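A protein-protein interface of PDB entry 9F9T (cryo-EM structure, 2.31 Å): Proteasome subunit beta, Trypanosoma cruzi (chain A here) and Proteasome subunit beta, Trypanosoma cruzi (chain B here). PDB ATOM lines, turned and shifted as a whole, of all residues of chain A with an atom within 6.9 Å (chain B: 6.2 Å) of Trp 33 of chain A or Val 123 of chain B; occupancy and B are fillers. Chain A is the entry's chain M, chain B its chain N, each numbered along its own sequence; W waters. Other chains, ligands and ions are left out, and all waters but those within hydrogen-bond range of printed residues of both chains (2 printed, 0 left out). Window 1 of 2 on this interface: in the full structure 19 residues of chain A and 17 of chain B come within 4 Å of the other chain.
Hydrophobic or aromatic side chains of chain A that line the printed part of chain B: Trp 33, Pro 35, Tyr 36, Met 89 and Ala 91. Hydrophobic or aromatic side chains of chain B within 4 Å of the printed part of chain A: Tyr 92, Phe 98, Pro 100, Leu 102 and Val 123. Along chain B the printed residues that touch a printed residue of chain A span positions 92 to 125. Among the printed residues, 17 pairs touch across the chains. Among the printed residues, Asp or Glu carboxylates within 4 Å of a Lys or Arg side-chain nitrogen of the other chain: Asp 92 of chain A with Arg 95 of chain B.
NH2 of Arg 95 of chain B is in hydrogen-bond range of O of Pro 35 of chain A, at 2.8 Å. NH2 of Arg 95 of chain B sits close to SD of Met 89 of chain A (3.8 Å). The side-chain hydroxyl of Tyr 92 of chain B lies within hydrogen-bond range of the side-chain carboxylate of Asp 92 of chain A (2.6 Å). The side-chain carboxylate (OD1) of Asp 92 of chain A lies within salt-bridge range of the guanidinium group (NH1) of Arg 95 of chain B (3.5 Å).
OG of Ser 34 of chain A lies close to N of Tyr 36 of chain A, 3.1 Å away. The backbone NH of Ala 37 of chain A lies within hydrogen-bond range of the side-chain sulfur of Met 89 of chain A (3.5 Å). The backbone carbonyl oxygen (O) of Gly 124 of chain B sits at hydrogen-bond distance from the side-chain amide nitrogen (NE2) of Gln 88 of chain B, at 3.0 Å. The side-chain hydroxyl of Tyr 92 of chain B lies within hydrogen-bond range of the guanidinium group of Arg 95 of chain B (3.5 Å). OG of Ser 96 of chain B sits at hydrogen-bond distance from O of Tyr 92 of chain B (3.2 Å). OD1 of Asp 121 of chain B lies within hydrogen-bond range of OG1 of Thr 125 of chain B, 2.9 Å away.
Trp 33 of chain A touches Arg 95 of chain B (CH2 to O, 3.7 Å). Trp 33 of chain A touches Pro 100 of chain B. Trp 33 of chain A touches Leu 102 of chain B. Trp 33 of chain A touches Val 123 of chain B. CG1 of Val 123 of chain B touches O of Ser 34 of chain A, at 3.5 Å. CE1 of Phe 98 of chain B touches CG of Pro 35 of chain A (3.6 Å). Tyr 36 of chain A touches Arg 95 of chain B. Ala 91 of chain A touches Val 123 of chain B. Gly 124 of chain B touches Ala 91 of chain A. Ala 91 of chain A touches Thr 125 of chain B (CB to N, 3.8 Å).
Printed residues of chain B within 4 Å of Trp 33 of chain A: Arg 95, Pro 100, Leu 102, Asp 122 and Val 123. Val 123 of chain B touches four residues of chain A. Of the printed residues of chain B, Ala 91 of chain A touches Tyr 92 (3.6 Å), Val 123 (3.5 Å), Gly 124 (3.6 Å) and Thr 125 (3.8 Å). Of the printed residues of chain B, Tyr 36 of chain A touches Arg 95. Of the printed residues of chain A, Thr 125 of chain B touches Ala 91 (3.8 Å). Cys 103 of chain B touches none of the printed residues of chain A. Ser 96 of chain B touches none of the printed residues of chain A. The nearest printed residue of chain B that does not touch Trp 33 of chain A is Phe 98 of chain B (4.01 Å). The nearest residue of chain A that does not touch Val 123 of chain B is Pro 35 of chain A (4.1 Å). The nearest printed residue of chain B that does not touch Pro 35 of chain A is Val 123 of chain B (4.1 Å).
Water W1 lies within hydrogen-bond range of OG1 of Thr 125 of chain B (2.4 Å), OD1 of Asn 39 of chain A (2.7 Å) and N of Ala 91 of chain A (3.1 Å). Water W2 lies within hydrogen-bond range of OD2 of Asp 92 of chain A and NH2 of Arg 95 of chain B.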
ATOM      1  N   TRP A  33     -15.894 -16.244 -18.274  1.00  0.00           N
ATOM      2  CA  TRP A  33     -15.582 -14.895 -17.716  1.00  0.00           C
ATOM      3  C   TRP A  33     -14.091 -14.643 -17.840  1.00  0.00           C
ATOM      4  O   TRP A  33     -13.318 -15.416 -17.292  1.00  0.00           O
ATOM      5  CB  TRP A  33     -15.974 -14.782 -16.244  1.00  0.00           C
ATOM      6  CG  TRP A  33     -15.657 -13.428 -15.654  1.00  0.00           C
ATOM      7  CD1 TRP A  33     -16.466 -12.338 -15.651  1.00  0.00           C
ATOM      8  CD2 TRP A  33     -14.450 -13.028 -14.979  1.00  0.00           C
ATOM      9  NE1 TRP A  33     -15.850 -11.292 -15.034  1.00  0.00           N
ATOM     10  CE2 TRP A  33     -14.617 -11.683 -14.609  1.00  0.00           C
ATOM     11  CE3 TRP A  33     -13.246 -13.668 -14.667  1.00  0.00           C
ATOM     12  CZ2 TRP A  33     -13.639 -10.961 -13.916  1.00  0.00           C
ATOM     13  CZ3 TRP A  33     -12.266 -12.960 -13.981  1.00  0.00           C
ATOM     14  CH2 TRP A  33     -12.473 -11.625 -13.590  1.00  0.00           C
ATOM     15  N   SER A  34     -13.733 -13.649 -18.668  1.00  0.00           N
ATOM     16  CA  SER A  34     -12.375 -13.130 -18.734  1.00  0.00           C
ATOM     17  C   SER A  34     -12.282 -11.853 -17.913  1.00  0.00           C
ATOM     18  O   SER A  34     -13.243 -11.133 -17.725  1.00  0.00           O
ATOM     19  CB  SER A  34     -11.949 -12.843 -20.128  1.00  0.00           C
ATOM     20  OG  SER A  34     -10.610 -12.333 -20.147  1.00  0.00           O
ATOM     21  N   PRO A  35     -11.110 -11.525 -17.379  1.00  0.00           N
ATOM     22  CA  PRO A  35     -10.939 -10.215 -16.759  1.00  0.00           C
ATOM     23  C   PRO A  35     -10.754  -9.086 -17.766  1.00  0.00           C
ATOM     24  O   PRO A  35     -10.579  -7.944 -17.343  1.00  0.00           O
ATOM     25  CB  PRO A  35      -9.757 -10.405 -15.805  1.00  0.00           C
ATOM     26  CG  PRO A  35      -8.999 -11.524 -16.486  1.00  0.00           C
ATOM     27  CD  PRO A  35     -10.011 -12.443 -17.136  1.00  0.00           C
ATOM     28  N   TYR A  36     -10.914  -9.400 -19.049  1.00  0.00           N
ATOM     29  CA  TYR A  36     -10.492  -8.518 -20.110  1.00  0.00           C
ATOM     30  C   TYR A  36     -11.664  -8.227 -21.020  1.00  0.00           C
ATOM     31  O   TYR A  36     -12.356  -9.129 -21.428  1.00  0.00           O
ATOM     32  CB  TYR A  36      -9.287  -9.108 -20.880  1.00  0.00           C
ATOM     33  CG  TYR A  36      -7.963  -9.026 -20.118  1.00  0.00           C
ATOM     34  CD1 TYR A  36      -7.551  -7.816 -19.587  1.00  0.00           C
ATOM     35  CD2 TYR A  36      -7.150 -10.129 -19.851  1.00  0.00           C
ATOM     36  CE1 TYR A  36      -6.338  -7.666 -18.916  1.00  0.00           C
ATOM     37  CE2 TYR A  36      -5.964 -10.008 -19.126  1.00  0.00           C
ATOM     38  CZ  TYR A  36      -5.528  -8.758 -18.674  1.00  0.00           C
ATOM     39  OH  TYR A  36      -4.351  -8.475 -17.988  1.00  0.00           O
ATOM     40  N   ALA A  37     -11.885  -6.969 -21.354  1.00  0.00           N
ATOM     41  CA  ALA A  37     -12.851  -6.574 -22.377  1.00  0.00           C
ATOM     42  C   ALA A  37     -12.172  -5.551 -23.266  1.00  0.00           C
ATOM     43  O   ALA A  37     -11.525  -4.683 -22.765  1.00  0.00           O
ATOM     44  CB  ALA A  37     -14.079  -5.942 -21.744  1.00  0.00           C
ATOM     45  N   ASN A  39     -13.138  -2.390 -25.367  1.00  0.00           N
ATOM     46  CA  ASN A  39     -14.252  -1.517 -25.616  1.00  0.00           C
ATOM     47  C   ASN A  39     -14.121  -0.743 -26.934  1.00  0.00           C
ATOM     48  O   ASN A  39     -14.965   0.090 -27.270  1.00  0.00           O
ATOM     49  CB  ASN A  39     -14.454  -0.660 -24.384  1.00  0.00           C
ATOM     50  CG  ASN A  39     -14.801  -1.519 -23.179  1.00  0.00           C
ATOM     51  OD1 ASN A  39     -14.066  -1.651 -22.196  1.00  0.00           O
ATOM     52  ND2 ASN A  39     -15.987  -2.079 -23.233  1.00  0.00           N
ATOM     53  N   MET A  89      -9.307  -1.659 -22.942  1.00  0.00           N
ATOM     54  CA  MET A  89     -10.325  -1.901 -21.971  1.00  0.00           C
ATOM     55  C   MET A  89     -10.527  -0.643 -21.149  1.00  0.00           C
ATOM     56  O   MET A  89      -9.636  -0.069 -20.560  1.00  0.00           O
ATOM     57  CB  MET A  89      -9.837  -3.043 -21.109  1.00  0.00           C
ATOM     58  CG  MET A  89     -10.706  -3.220 -19.942  1.00  0.00           C
ATOM     59  SD  MET A  89     -10.282  -4.731 -19.156  1.00  0.00           S
ATOM     60  CE  MET A  89     -11.550  -4.874 -17.920  1.00  0.00           C
ATOM     61  N   ALA A  91     -12.071  -0.106 -18.301  1.00  0.00           N
ATOM     62  CA  ALA A  91     -11.961  -0.067 -16.864  1.00  0.00           C
ATOM     63  C   ALA A  91     -10.500   0.058 -16.448  1.00  0.00           C
ATOM     64  O   ALA A  91     -10.223   0.518 -15.349  1.00  0.00           O
ATOM     65  CB  ALA A  91     -12.539  -1.300 -16.247  1.00  0.00           C
ATOM     66  N   ASP A  92      -9.615  -0.495 -17.283  1.00  0.00           N
ATOM     67  CA  ASP A  92      -8.195  -0.422 -17.073  1.00  0.00           C
ATOM     68  C   ASP A  92      -7.702   0.988 -17.290  1.00  0.00           C
ATOM     69  O   ASP A  92      -7.023   1.509 -16.428  1.00  0.00           O
ATOM     70  CB  ASP A  92      -7.430  -1.455 -17.914  1.00  0.00           C
ATOM     71  CG  ASP A  92      -7.308  -2.806 -17.234  1.00  0.00           C
ATOM     72  OD1 ASP A  92      -7.946  -2.982 -16.168  1.00  0.00           O
ATOM     73  OD2 ASP A  92      -6.618  -3.686 -17.768  1.00  0.00           O
ATOM     74  N   GLN B  88     -18.322   1.188  -8.638  1.00  0.00           N
ATOM     75  CA  GLN B  88     -17.436   0.812  -9.734  1.00  0.00           C
ATOM     76  C   GLN B  88     -16.034   0.437  -9.244  1.00  0.00           C
ATOM     77  O   GLN B  88     -15.450  -0.497  -9.689  1.00  0.00           O
ATOM     78  CB  GLN B  88     -17.374   1.927 -10.774  1.00  0.00           C
ATOM     79  CG  GLN B  88     -16.528   1.575 -11.991  1.00  0.00           C
ATOM     80  CD  GLN B  88     -15.023   1.761 -11.855  1.00  0.00           C
ATOM     81  OE1 GLN B  88     -14.512   2.590 -11.125  1.00  0.00           O
ATOM     82  NE2 GLN B  88     -14.271   0.959 -12.563  1.00  0.00           N
ATOM     83  N   VAL B  91     -16.508  -3.250  -7.801  1.00  0.00           N
ATOM     84  CA  VAL B  91     -16.578  -4.145  -8.916  1.00  0.00           C
ATOM     85  C   VAL B  91     -15.217  -4.354  -9.519  1.00  0.00           C
ATOM     86  O   VAL B  91     -14.861  -5.489  -9.780  1.00  0.00           O
ATOM     87  CB  VAL B  91     -17.543  -3.660  -9.949  1.00  0.00           C
ATOM     88  CG1 VAL B  91     -17.508  -4.639 -11.149  1.00  0.00           C
ATOM     89  CG2 VAL B  91     -18.936  -3.603  -9.336  1.00  0.00           C
ATOM     90  N   TYR B  92     -14.445  -3.299  -9.671  1.00  0.00           N
ATOM     91  CA  TYR B  92     -13.164  -3.386 -10.352  1.00  0.00           C
ATOM     92  C   TYR B  92     -12.138  -4.156  -9.540  1.00  0.00           C
ATOM     93  O   TYR B  92     -11.399  -4.944 -10.054  1.00  0.00           O
ATOM     94  CB  TYR B  92     -12.581  -1.994 -10.626  1.00  0.00           C
ATOM     95  CG  TYR B  92     -11.264  -2.050 -11.376  1.00  0.00           C
ATOM     96  CD1 TYR B  92     -11.265  -2.413 -12.707  1.00  0.00           C
ATOM     97  CD2 TYR B  92     -10.026  -1.812 -10.766  1.00  0.00           C
ATOM     98  CE1 TYR B  92     -10.079  -2.501 -13.414  1.00  0.00           C
ATOM     99  CE2 TYR B  92      -8.829  -1.938 -11.480  1.00  0.00           C
ATOM    100  CZ  TYR B  92      -8.885  -2.184 -12.826  1.00  0.00           C
ATOM    101  OH  TYR B  92      -7.889  -2.313 -13.694  1.00  0.00           O
ATOM    102  N   LYS B  94     -12.656  -6.446  -7.300  1.00  0.00           N
ATOM    103  CA  LYS B  94     -12.941  -7.854  -7.279  1.00  0.00           C
ATOM    104  C   LYS B  94     -12.563  -8.549  -8.543  1.00  0.00           C
ATOM    105  O   LYS B  94     -12.151  -9.683  -8.499  1.00  0.00           O
ATOM    106  CB  LYS B  94     -14.443  -8.018  -7.082  1.00  0.00           C
ATOM    107  CG  LYS B  94     -14.898  -7.704  -5.675  1.00  0.00           C
ATOM    108  CD  LYS B  94     -16.349  -8.051  -5.547  1.00  0.00           C
ATOM    109  CE  LYS B  94     -16.678  -8.876  -4.317  1.00  0.00           C
ATOM    110  NZ  LYS B  94     -18.037  -8.506  -3.807  1.00  0.00           N
ATOM    111  N   ARG B  95     -12.803  -7.899  -9.679  1.00  0.00           N
ATOM    112  CA  ARG B  95     -12.311  -8.383 -10.948  1.00  0.00           C
ATOM    113  C   ARG B  95     -10.796  -8.554 -10.937  1.00  0.00           C
ATOM    114  O   ARG B  95     -10.270  -9.522 -11.435  1.00  0.00           O
ATOM    115  CB  ARG B  95     -12.738  -7.399 -12.038  1.00  0.00           C
ATOM    116  CG  ARG B  95     -12.040  -7.585 -13.371  1.00  0.00           C
ATOM    117  CD  ARG B  95     -10.824  -6.702 -13.469  1.00  0.00           C
ATOM    118  NE  ARG B  95     -10.201  -6.866 -14.775  1.00  0.00           N
ATOM    119  CZ  ARG B  95      -9.025  -6.368 -15.045  1.00  0.00           C
ATOM    120  NH1 ARG B  95      -8.339  -5.741 -14.122  1.00  0.00           N
ATOM    121  NH2 ARG B  95      -8.547  -6.423 -16.262  1.00  0.00           N
ATOM    122  N   SER B  96     -10.126  -7.664 -10.252  1.00  0.00           N
ATOM    123  CA  SER B  96      -8.685  -7.633 -10.215  1.00  0.00           C
ATOM    124  C   SER B  96      -8.122  -8.732  -9.320  1.00  0.00           C
ATOM    125  O   SER B  96      -6.999  -9.209  -9.558  1.00  0.00           O
ATOM    126  CB  SER B  96      -8.191  -6.209  -9.867  1.00  0.00           C
ATOM    127  OG  SER B  96      -8.369  -5.361 -11.010  1.00  0.00           O
ATOM    128  N   PHE B  98      -9.742 -11.690  -9.483  1.00  0.00           N
ATOM    129  CA  PHE B  98     -10.316 -12.891 -10.090  1.00  0.00           C
ATOM    130  C   PHE B  98     -11.364 -13.516  -9.186  1.00  0.00           C
ATOM    131  O   PHE B  98     -11.426 -14.723  -9.066  1.00  0.00           O
ATOM    132  CB  PHE B  98      -9.249 -13.947 -10.378  1.00  0.00           C
ATOM    133  CG  PHE B  98      -8.266 -13.521 -11.422  1.00  0.00           C
ATOM    134  CD1 PHE B  98      -8.527 -13.759 -12.764  1.00  0.00           C
ATOM    135  CD2 PHE B  98      -7.119 -12.833 -11.068  1.00  0.00           C
ATOM    136  CE1 PHE B  98      -7.632 -13.330 -13.735  1.00  0.00           C
ATOM    137  CE2 PHE B  98      -6.257 -12.358 -12.043  1.00  0.00           C
ATOM    138  CZ  PHE B  98      -6.499 -12.625 -13.376  1.00  0.00           C
ATOM    139  N   GLU B  99     -12.181 -12.694  -8.557  1.00  0.00           N
ATOM    140  CA  GLU B  99     -13.338 -13.119  -7.784  1.00  0.00           C
ATOM    141  C   GLU B  99     -14.462 -12.173  -8.133  1.00  0.00           C
ATOM    142  O   GLU B  99     -14.844 -11.306  -7.349  1.00  0.00           O
ATOM    143  CB  GLU B  99     -13.040 -12.979  -6.289  1.00  0.00           C
ATOM    144  CG  GLU B  99     -11.708 -13.634  -5.872  1.00  0.00           C
ATOM    145  CD  GLU B  99     -11.410 -13.621  -4.375  1.00  0.00           C
ATOM    146  OE1 GLU B  99     -11.426 -12.517  -3.760  1.00  0.00           O
ATOM    147  OE2 GLU B  99     -11.152 -14.715  -3.817  1.00  0.00           O
ATOM    148  N   PRO B 100     -14.878 -12.134  -9.394  1.00  0.00           N
ATOM    149  CA  PRO B 100     -15.785 -11.080  -9.818  1.00  0.00           C
ATOM    150  C   PRO B 100     -17.191 -11.092  -9.219  1.00  0.00           C
ATOM    151  O   PRO B 100     -17.712 -12.137  -8.831  1.00  0.00           O
ATOM    152  CB  PRO B 100     -15.967 -11.364 -11.287  1.00  0.00           C
ATOM    153  CG  PRO B 100     -15.633 -12.836 -11.403  1.00  0.00           C
ATOM    154  CD  PRO B 100     -14.486 -13.029 -10.461  1.00  0.00           C
ATOM    155  N   CYS B 101     -17.771  -9.913  -9.196  1.00  0.00           N
ATOM    156  CA  CYS B 101     -19.187  -9.729  -9.007  1.00  0.00           C
ATOM    157  C   CYS B 101     -19.894 -10.061 -10.317  1.00  0.00           C
ATOM    158  O   CYS B 101     -19.856  -9.264 -11.226  1.00  0.00           O
ATOM    159  CB  CYS B 101     -19.375  -8.268  -8.627  1.00  0.00           C
ATOM    160  SG  CYS B 101     -20.973  -7.891  -7.867  1.00  0.00           S
ATOM    161  N   LEU B 102     -20.491 -11.234 -10.470  1.00  0.00           N
ATOM    162  CA  LEU B 102     -21.037 -11.609 -11.766  1.00  0.00           C
ATOM    163  C   LEU B 102     -22.411 -10.953 -11.969  1.00  0.00           C
ATOM    164  O   LEU B 102     -23.413 -11.632 -12.116  1.00  0.00           O
ATOM    165  CB  LEU B 102     -21.074 -13.141 -11.892  1.00  0.00           C
ATOM    166  CG  LEU B 102     -19.699 -13.831 -11.993  1.00  0.00           C
ATOM    167  CD1 LEU B 102     -19.859 -15.341 -12.051  1.00  0.00           C
ATOM    168  CD2 LEU B 102     -18.884 -13.377 -13.192  1.00  0.00           C
ATOM    169  N   CYS B 103     -22.431  -9.611 -11.960  1.00  0.00           N
ATOM    170  CA  CYS B 103     -23.641  -8.838 -12.204  1.00  0.00           C
ATOM    171  C   CYS B 103     -23.349  -7.670 -13.088  1.00  0.00           C
ATOM    172  O   CYS B 103     -22.213  -7.291 -13.201  1.00  0.00           O
ATOM    173  CB  CYS B 103     -24.100  -7.968 -11.059  1.00  0.00           C
ATOM    174  SG  CYS B 103     -24.598  -8.878  -9.609  1.00  0.00           S
ATOM    175  N   ASP B 121     -20.476  -2.753 -15.630  1.00  0.00           N
ATOM    176  CA  ASP B 121     -20.446  -4.168 -15.880  1.00  0.00           C
ATOM    177  C   ASP B 121     -19.425  -4.942 -15.052  1.00  0.00           C
ATOM    178  O   ASP B 121     -18.723  -4.375 -14.241  1.00  0.00           O
ATOM    179  CB  ASP B 121     -20.276  -4.438 -17.335  1.00  0.00           C
ATOM    180  CG  ASP B 121     -18.876  -4.351 -17.836  1.00  0.00           C
ATOM    181  OD1 ASP B 121     -17.949  -4.035 -17.011  1.00  0.00           O
ATOM    182  OD2 ASP B 121     -18.686  -4.619 -19.021  1.00  0.00           O
ATOM    183  N   ASP B 122     -19.355  -6.262 -15.209  1.00  0.00           N
ATOM    184  CA  ASP B 122     -18.677  -7.099 -14.220  1.00  0.00           C
ATOM    185  C   ASP B 122     -17.148  -7.046 -14.349  1.00  0.00           C
ATOM    186  O   ASP B 122     -16.412  -7.558 -13.505  1.00  0.00           O
ATOM    187  CB  ASP B 122     -19.147  -8.540 -14.326  1.00  0.00           C
ATOM    188  CG  ASP B 122     -18.803  -9.203 -15.666  1.00  0.00           C
ATOM    189  OD1 ASP B 122     -19.437 -10.246 -16.006  1.00  0.00           O
ATOM    190  OD2 ASP B 122     -17.925  -8.710 -16.374  1.00  0.00           O
ATOM    191  N   VAL B 123     -16.628  -6.392 -15.377  1.00  0.00           N
ATOM    192  CA  VAL B 123     -15.209  -6.156 -15.273  1.00  0.00           C
ATOM    193  C   VAL B 123     -14.953  -4.715 -14.854  1.00  0.00           C
ATOM    194  O   VAL B 123     -13.824  -4.340 -14.973  1.00  0.00           O
ATOM    195  CB  VAL B 123     -14.481  -6.504 -16.573  1.00  0.00           C
ATOM    196  CG1 VAL B 123     -14.643  -7.991 -16.896  1.00  0.00           C
ATOM    197  CG2 VAL B 123     -15.014  -5.660 -17.718  1.00  0.00           C
ATOM    198  N   GLY B 124     -15.966  -3.911 -14.471  1.00  0.00           N
ATOM    199  CA  GLY B 124     -15.704  -2.545 -14.039  1.00  0.00           C
ATOM    200  C   GLY B 124     -15.963  -1.442 -15.083  1.00  0.00           C
ATOM    201  O   GLY B 124     -15.887  -0.290 -14.704  1.00  0.00           O
ATOM    202  N   THR B 125     -16.305  -1.742 -16.344  1.00  0.00           N
ATOM    203  CA  THR B 125     -16.751  -0.742 -17.314  1.00  0.00           C
ATOM    204  C   THR B 125     -17.913   0.111 -16.822  1.00  0.00           C
ATOM    205  O   THR B 125     -18.901  -0.464 -16.383  1.00  0.00           O
ATOM    206  CB  THR B 125     -17.247  -1.396 -18.593  1.00  0.00           C
ATOM    207  OG1 THR B 125     -16.394  -2.487 -18.887  1.00  0.00           O
ATOM    208  CG2 THR B 125     -17.324  -0.467 -19.787  1.00  0.00           C
HETATM  209  O   HOH W   1     -14.092  -2.116 -19.532  1.00  0.00           O
HETATM  210  O   HOH W   2      -5.259  -5.448 -16.120  1.00  0.00           O
